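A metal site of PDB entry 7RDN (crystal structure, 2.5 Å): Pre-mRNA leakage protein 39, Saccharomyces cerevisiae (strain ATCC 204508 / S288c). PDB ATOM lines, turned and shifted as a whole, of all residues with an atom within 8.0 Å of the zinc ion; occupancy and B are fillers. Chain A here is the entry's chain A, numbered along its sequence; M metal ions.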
ATOM      1  N   LYS A  47      10.573  36.033 -31.184  1.00  0.00           N
ATOM      2  CA  LYS A  47      10.735  35.068 -30.103  1.00  0.00           C
ATOM      3  C   LYS A  47      11.017  33.653 -30.622  1.00  0.00           C
ATOM      4  O   LYS A  47      10.739  32.671 -29.924  1.00  0.00           O
ATOM      5  CB  LYS A  47       9.509  35.083 -29.194  1.00  0.00           C
ATOM      6  CG  LYS A  47       9.311  36.419 -28.479  1.00  0.00           C
ATOM      7  CD  LYS A  47      10.438  36.734 -27.498  1.00  0.00           C
ATOM      8  CE  LYS A  47      10.398  35.836 -26.278  1.00  0.00           C
ATOM      9  NZ  LYS A  47      11.525  36.085 -25.344  1.00  0.00           N
ATOM     10  N   GLY A  48      11.566  33.536 -31.826  1.00  0.00           N
ATOM     11  CA  GLY A  48      12.051  32.273 -32.328  1.00  0.00           C
ATOM     12  C   GLY A  48      10.996  31.294 -32.776  1.00  0.00           C
ATOM     13  O   GLY A  48      11.326  30.124 -33.032  1.00  0.00           O
ATOM     14  N   TRP A  49       9.744  31.715 -32.904  1.00  0.00           N
ATOM     15  CA  TRP A  49       8.679  30.813 -33.284  1.00  0.00           C
ATOM     16  C   TRP A  49       8.595  30.669 -34.798  1.00  0.00           C
ATOM     17  O   TRP A  49       8.750  31.652 -35.539  1.00  0.00           O
ATOM     18  CB  TRP A  49       7.336  31.288 -32.712  1.00  0.00           C
ATOM     19  CG  TRP A  49       7.291  31.158 -31.212  1.00  0.00           C
ATOM     20  CD1 TRP A  49       7.498  32.145 -30.286  1.00  0.00           C
ATOM     21  CD2 TRP A  49       7.036  29.965 -30.468  1.00  0.00           C
ATOM     22  NE1 TRP A  49       7.378  31.639 -29.019  1.00  0.00           N
ATOM     23  CE2 TRP A  49       7.102  30.297 -29.101  1.00  0.00           C
ATOM     24  CE3 TRP A  49       6.763  28.636 -30.825  1.00  0.00           C
ATOM     25  CZ2 TRP A  49       6.901  29.358 -28.085  1.00  0.00           C
ATOM     26  CZ3 TRP A  49       6.558  27.708 -29.817  1.00  0.00           C
ATOM     27  CH2 TRP A  49       6.631  28.070 -28.461  1.00  0.00           C
ATOM     28  N   LYS A  63       6.076  26.279 -33.454  1.00  0.00           N
ATOM     29  CA  LYS A  63       7.120  25.508 -32.789  1.00  0.00           C
ATOM     30  C   LYS A  63       8.377  26.357 -32.695  1.00  0.00           C
ATOM     31  O   LYS A  63       8.721  27.076 -33.625  1.00  0.00           O
ATOM     32  CB  LYS A  63       7.395  24.217 -33.558  1.00  0.00           C
ATOM     33  CG  LYS A  63       8.415  23.290 -32.928  1.00  0.00           C
ATOM     34  CD  LYS A  63       8.590  22.040 -33.782  1.00  0.00           C
ATOM     35  CE  LYS A  63       9.664  21.113 -33.235  1.00  0.00           C
ATOM     36  NZ  LYS A  63       9.966  19.972 -34.149  1.00  0.00           N
ATOM     37  N   CYS A  64       9.052  26.266 -31.547  1.00  0.00           N
ATOM     38  CA  CYS A  64      10.276  27.030 -31.363  1.00  0.00           C
ATOM     39  C   CYS A  64      11.451  26.324 -32.037  1.00  0.00           C
ATOM     40  O   CYS A  64      11.612  25.105 -31.920  1.00  0.00           O
ATOM     41  CB  CYS A  64      10.573  27.228 -29.878  1.00  0.00           C
ATOM     42  SG  CYS A  64      12.257  27.773 -29.545  1.00  0.00           S
ATOM     43  N   CYS A  65      12.275  27.107 -32.732  1.00  0.00           N
ATOM     44  CA  CYS A  65      13.385  26.528 -33.486  1.00  0.00           C
ATOM     45  C   CYS A  65      14.460  25.936 -32.595  1.00  0.00           C
ATOM     46  O   CYS A  65      15.308  25.191 -33.104  1.00  0.00           O
ATOM     47  CB  CYS A  65      13.974  27.587 -34.416  1.00  0.00           C
ATOM     48  SG  CYS A  65      14.567  29.098 -33.608  1.00  0.00           S
ATOM     49  N   CYS A  66      14.462  26.232 -31.301  1.00  0.00           N
ATOM     50  CA  CYS A  66      15.410  25.654 -30.350  1.00  0.00           C
ATOM     51  C   CYS A  66      14.746  24.701 -29.367  1.00  0.00           C
ATOM     52  O   CYS A  66      15.198  23.561 -29.217  1.00  0.00           O
ATOM     53  CB  CYS A  66      16.141  26.773 -29.590  1.00  0.00           C
ATOM     54  SG  CYS A  66      17.158  27.833 -30.635  1.00  0.00           S
ATOM     55  N   CYS A  67      13.696  25.147 -28.686  1.00  0.00           N
ATOM     56  CA  CYS A  67      12.976  24.268 -27.762  1.00  0.00           C
ATOM     57  C   CYS A  67      12.431  23.048 -28.478  1.00  0.00           C
ATOM     58  O   CYS A  67      12.622  21.909 -28.031  1.00  0.00           O
ATOM     59  CB  CYS A  67      11.824  25.013 -27.096  1.00  0.00           C
ATOM     60  SG  CYS A  67      12.233  25.958 -25.648  1.00  0.00           S
ATOM     61  N   HIS A  68      11.739  23.260 -29.594  1.00  0.00           N
ATOM     62  CA  HIS A  68      10.791  22.329 -30.197  1.00  0.00           C
ATOM     63  C   HIS A  68       9.485  22.315 -29.409  1.00  0.00           C
ATOM     64  O   HIS A  68       8.660  21.406 -29.620  1.00  0.00           O
ATOM     65  CB  HIS A  68      11.379  20.917 -30.299  1.00  0.00           C
ATOM     66  CG  HIS A  68      12.752  20.897 -30.907  1.00  0.00           C
ATOM     67  ND1 HIS A  68      12.990  21.267 -32.213  1.00  0.00           N
ATOM     68  CD2 HIS A  68      13.955  20.562 -30.387  1.00  0.00           C
ATOM     69  CE1 HIS A  68      14.281  21.158 -32.473  1.00  0.00           C
ATOM     70  NE2 HIS A  68      14.883  20.727 -31.374  1.00  0.00           N
ATOM     71  N   ALA A  69       9.284  23.272 -28.519  1.00  0.00           N
ATOM     72  CA  ALA A  69       8.027  23.407 -27.785  1.00  0.00           C
ATOM     73  C   ALA A  69       6.956  24.010 -28.689  1.00  0.00           C
ATOM     74  O   ALA A  69       7.247  24.747 -29.630  1.00  0.00           O
ATOM     75  CB  ALA A  69       8.221  24.279 -26.549  1.00  0.00           C
ATOM     76  N   ILE A  70       5.697  23.714 -28.363  1.00  0.00           N
ATOM     77  CA  ILE A  70       4.565  24.047 -29.216  1.00  0.00           C
ATOM     78  C   ILE A  70       3.690  25.073 -28.509  1.00  0.00           C
ATOM     79  O   ILE A  70       3.444  24.976 -27.307  1.00  0.00           O
ATOM     80  CB  ILE A  70       3.743  22.783 -29.561  1.00  0.00           C
ATOM     81  CG1 ILE A  70       4.659  21.637 -30.004  1.00  0.00           C
ATOM     82  CG2 ILE A  70       2.733  23.109 -30.649  1.00  0.00           C
ATOM     83  CD1 ILE A  70       5.546  21.977 -31.188  1.00  0.00           C
ATOM     84  N   ILE A  98       4.016  32.880 -26.094  1.00  0.00           N
ATOM     85  CA  ILE A  98       5.158  33.304 -26.897  1.00  0.00           C
ATOM     86  C   ILE A  98       6.419  33.327 -26.040  1.00  0.00           C
ATOM     87  O   ILE A  98       7.513  33.021 -26.521  1.00  0.00           O
ATOM     88  CB  ILE A  98       4.856  34.668 -27.545  1.00  0.00           C
ATOM     89  CG1 ILE A  98       3.562  34.594 -28.354  1.00  0.00           C
ATOM     90  CG2 ILE A  98       6.004  35.089 -28.449  1.00  0.00           C
ATOM     91  CD1 ILE A  98       3.254  35.822 -29.178  1.00  0.00           C
ATOM     92  N   ILE A  99       6.287  33.683 -24.759  1.00  0.00           N
ATOM     93  CA  ILE A  99       7.380  33.580 -23.794  1.00  0.00           C
ATOM     94  C   ILE A  99       7.278  32.289 -22.985  1.00  0.00           C
ATOM     95  O   ILE A  99       8.248  31.536 -22.880  1.00  0.00           O
ATOM     96  CB  ILE A  99       7.396  34.806 -22.862  1.00  0.00           C
ATOM     97  CG1 ILE A  99       7.750  36.078 -23.630  1.00  0.00           C
ATOM     98  CG2 ILE A  99       8.368  34.593 -21.719  1.00  0.00           C
ATOM     99  CD1 ILE A  99       7.521  37.361 -22.844  1.00  0.00           C
ATOM    100  N   GLY A 100       6.107  32.030 -22.397  1.00  0.00           N
ATOM    101  CA  GLY A 100       6.010  30.986 -21.393  1.00  0.00           C
ATOM    102  C   GLY A 100       6.264  29.588 -21.940  1.00  0.00           C
ATOM    103  O   GLY A 100       6.965  28.786 -21.302  1.00  0.00           O
ATOM    104  N   ASN A 101       5.720  29.277 -23.108  1.00  0.00           N
ATOM    105  CA  ASN A 101       5.828  27.917 -23.628  1.00  0.00           C
ATOM    106  C   ASN A 101       7.268  27.503 -23.893  1.00  0.00           C
ATOM    107  O   ASN A 101       7.546  26.310 -24.024  1.00  0.00           O
ATOM    108  CB  ASN A 101       5.002  27.766 -24.902  1.00  0.00           C
ATOM    109  CG  ASN A 101       3.514  27.669 -24.624  1.00  0.00           C
ATOM    110  OD1 ASN A 101       3.049  28.101 -23.573  1.00  0.00           O
ATOM    111  ND2 ASN A 101       2.771  27.103 -25.568  1.00  0.00           N
ATOM    112  N   HIS A 102       8.199  28.462 -23.967  1.00  0.00           N
ATOM    113  CA  HIS A 102       9.604  28.106 -24.128  1.00  0.00           C
ATOM    114  C   HIS A 102      10.089  27.317 -22.922  1.00  0.00           C
ATOM    115  O   HIS A 102       9.704  27.589 -21.782  1.00  0.00           O
ATOM    116  CB  HIS A 102      10.455  29.367 -24.292  1.00  0.00           C
ATOM    117  CG  HIS A 102      10.336  29.996 -25.649  1.00  0.00           C
ATOM    118  ND1 HIS A 102      10.894  29.445 -26.780  1.00  0.00           N
ATOM    119  CD2 HIS A 102       9.724  31.139 -26.045  1.00  0.00           C
ATOM    120  CE1 HIS A 102      10.634  30.218 -27.820  1.00  0.00           C
ATOM    121  NE2 HIS A 102       9.923  31.245 -27.396  1.00  0.00           N
ATOM    122  N   LEU A 103      10.948  26.336 -23.180  1.00  0.00           N
ATOM    123  CA  LEU A 103      11.577  25.598 -22.092  1.00  0.00           C
ATOM    124  C   LEU A 103      12.420  26.564 -21.249  1.00  0.00           C
ATOM    125  O   LEU A 103      12.864  27.615 -21.718  1.00  0.00           O
ATOM    126  CB  LEU A 103      12.446  24.469 -22.646  1.00  0.00           C
ATOM    127  CG  LEU A 103      11.679  23.395 -23.411  1.00  0.00           C
ATOM    128  CD1 LEU A 103      12.624  22.393 -24.051  1.00  0.00           C
ATOM    129  CD2 LEU A 103      10.693  22.676 -22.495  1.00  0.00           C
ATOM    130  N   GLN A 104      12.621  26.185 -19.983  1.00  0.00           N
ATOM    131  CA  GLN A 104      13.132  27.135 -19.006  1.00  0.00           C
ATOM    132  C   GLN A 104      14.475  27.731 -19.428  1.00  0.00           C
ATOM    133  O   GLN A 104      14.702  28.931 -19.256  1.00  0.00           O
ATOM    134  CB  GLN A 104      13.257  26.465 -17.635  1.00  0.00           C
ATOM    135  CG  GLN A 104      13.148  27.424 -16.455  1.00  0.00           C
ATOM    136  CD  GLN A 104      11.787  28.108 -16.397  1.00  0.00           C
ATOM    137  OE1 GLN A 104      10.756  27.465 -16.539  1.00  0.00           O
ATOM    138  NE2 GLN A 104      11.801  29.427 -16.201  1.00  0.00           N
ATOM    139  N   LYS A 105      15.358  26.914 -19.985  1.00  0.00           N
ATOM    140  CA  LYS A 105      16.702  27.351 -20.328  1.00  0.00           C
ATOM    141  C   LYS A 105      16.879  27.644 -21.811  1.00  0.00           C
ATOM    142  O   LYS A 105      18.018  27.855 -22.256  1.00  0.00           O
ATOM    143  CB  LYS A 105      17.721  26.299 -19.887  1.00  0.00           C
ATOM    144  CG  LYS A 105      17.924  26.255 -18.385  1.00  0.00           C
ATOM    145  CD  LYS A 105      19.010  25.279 -17.997  1.00  0.00           C
ATOM    146  CE  LYS A 105      19.226  25.264 -16.498  1.00  0.00           C
ATOM    147  NZ  LYS A 105      20.226  24.237 -16.089  1.00  0.00           N
ATOM    148  N   CYS A 106      15.811  27.667 -22.579  1.00  0.00           N
ATOM    149  CA  CYS A 106      15.934  28.012 -23.984  1.00  0.00           C
ATOM    150  C   CYS A 106      16.295  29.492 -24.123  1.00  0.00           C
ATOM    151  O   CYS A 106      15.761  30.338 -23.400  1.00  0.00           O
ATOM    152  CB  CYS A 106      14.627  27.730 -24.713  1.00  0.00           C
ATOM    153  SG  CYS A 106      14.416  28.650 -26.250  1.00  0.00           S
ATOM    154  N   PRO A 107      17.193  29.829 -25.050  1.00  0.00           N
ATOM    155  CA  PRO A 107      17.597  31.241 -25.168  1.00  0.00           C
ATOM    156  C   PRO A 107      16.461  32.181 -25.518  1.00  0.00           C
ATOM    157  O   PRO A 107      16.520  33.359 -25.160  1.00  0.00           O
ATOM    158  CB  PRO A 107      18.666  31.205 -26.280  1.00  0.00           C
ATOM    159  CG  PRO A 107      18.388  29.950 -27.040  1.00  0.00           C
ATOM    160  CD  PRO A 107      17.863  28.967 -26.041  1.00  0.00           C
ATOM    161  N   TRP A 108      15.423  31.695 -26.190  1.00  0.00           N
ATOM    162  CA  TRP A 108      14.328  32.564 -26.615  1.00  0.00           C
ATOM    163  C   TRP A 108      13.407  32.973 -25.472  1.00  0.00           C
ATOM    164  O   TRP A 108      12.627  33.918 -25.640  1.00  0.00           O
ATOM    165  CB  TRP A 108      13.507  31.892 -27.719  1.00  0.00           C
ATOM    166  CG  TRP A 108      14.222  31.791 -29.037  1.00  0.00           C
ATOM    167  CD1 TRP A 108      14.682  30.651 -29.633  1.00  0.00           C
ATOM    168  CD2 TRP A 108      14.541  32.864 -29.925  1.00  0.00           C
ATOM    169  NE1 TRP A 108      15.267  30.954 -30.835  1.00  0.00           N
ATOM    170  CE2 TRP A 108      15.203  32.298 -31.040  1.00  0.00           C
ATOM    171  CE3 TRP A 108      14.345  34.248 -29.896  1.00  0.00           C
ATOM    172  CZ2 TRP A 108      15.653  33.074 -32.110  1.00  0.00           C
ATOM    173  CZ3 TRP A 108      14.798  35.013 -30.958  1.00  0.00           C
ATOM    174  CH2 TRP A 108      15.452  34.425 -32.047  1.00  0.00           C
ATOM    175  N   ARG A 109      13.453  32.282 -24.329  1.00  0.00           N
ATOM    176  CA  ARG A 109      12.532  32.605 -23.249  1.00  0.00           C
ATOM    177  C   ARG A 109      12.782  34.002 -22.698  1.00  0.00           C
ATOM    178  O   ARG A 109      11.846  34.801 -22.554  1.00  0.00           O
ATOM    179  CB  ARG A 109      12.652  31.561 -22.131  1.00  0.00           C
ATOM    180  CG  ARG A 109      11.642  31.760 -21.004  1.00  0.00           C
ATOM    181  CD  ARG A 109      11.775  30.688 -19.935  1.00  0.00           C
ATOM    182  NE  ARG A 109      10.791  30.860 -18.877  1.00  0.00           N
ATOM    183  CZ  ARG A 109       9.541  30.401 -18.920  1.00  0.00           C
ATOM    184  NH1 ARG A 109       9.083  29.755 -19.986  1.00  0.00           N
ATOM    185  NH2 ARG A 109       8.736  30.610 -17.885  1.00  0.00           N
HETATM  186 ZN    ZN M   1      12.167  27.739 -27.187  1.00  0.00          ZN
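O of His 102 lies within hydrogen-bond range of NH1 of Arg 109, at 2.9 Å. The indole nitrogen (NE1) of Trp 49 lies within hydrogen-bond range of a ring nitrogen (NE2) of His 102, at 3.0 Å. The backbone carbonyl oxygen of Lys 47 is in hydrogen-bond range of a ring nitrogen (NE2) of His 102. NE2 of His 102 lies close to O of Ile 98 (3.1 Å). The backbone NH (N) of Leu 103 lies close to the side-chain sulfur (SG) of Cys 67 (2.8 Å). SG of Cys 64 lies close to N of Cys 66, at 3.2 Å. O of Ala 69 sits at hydrogen-bond distance from N of Cys 64 (3.0 Å). The side-chain sulfur (SG) of Cys 106 sits close to the backbone NH (N) of Trp 108.
Within 4 Å of the zinc ion: Cys 64, Cys 67, His 102 and Cys 106.
The zinc ion is bound by ND1 of His 102 (2.2 Å), SG of Cys 67 (2.4 Å), SG of Cys 64 (2.4 Å) and SG of Cys 106 (2.6 Å). The zinc ion has four donor atoms within binding distance.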
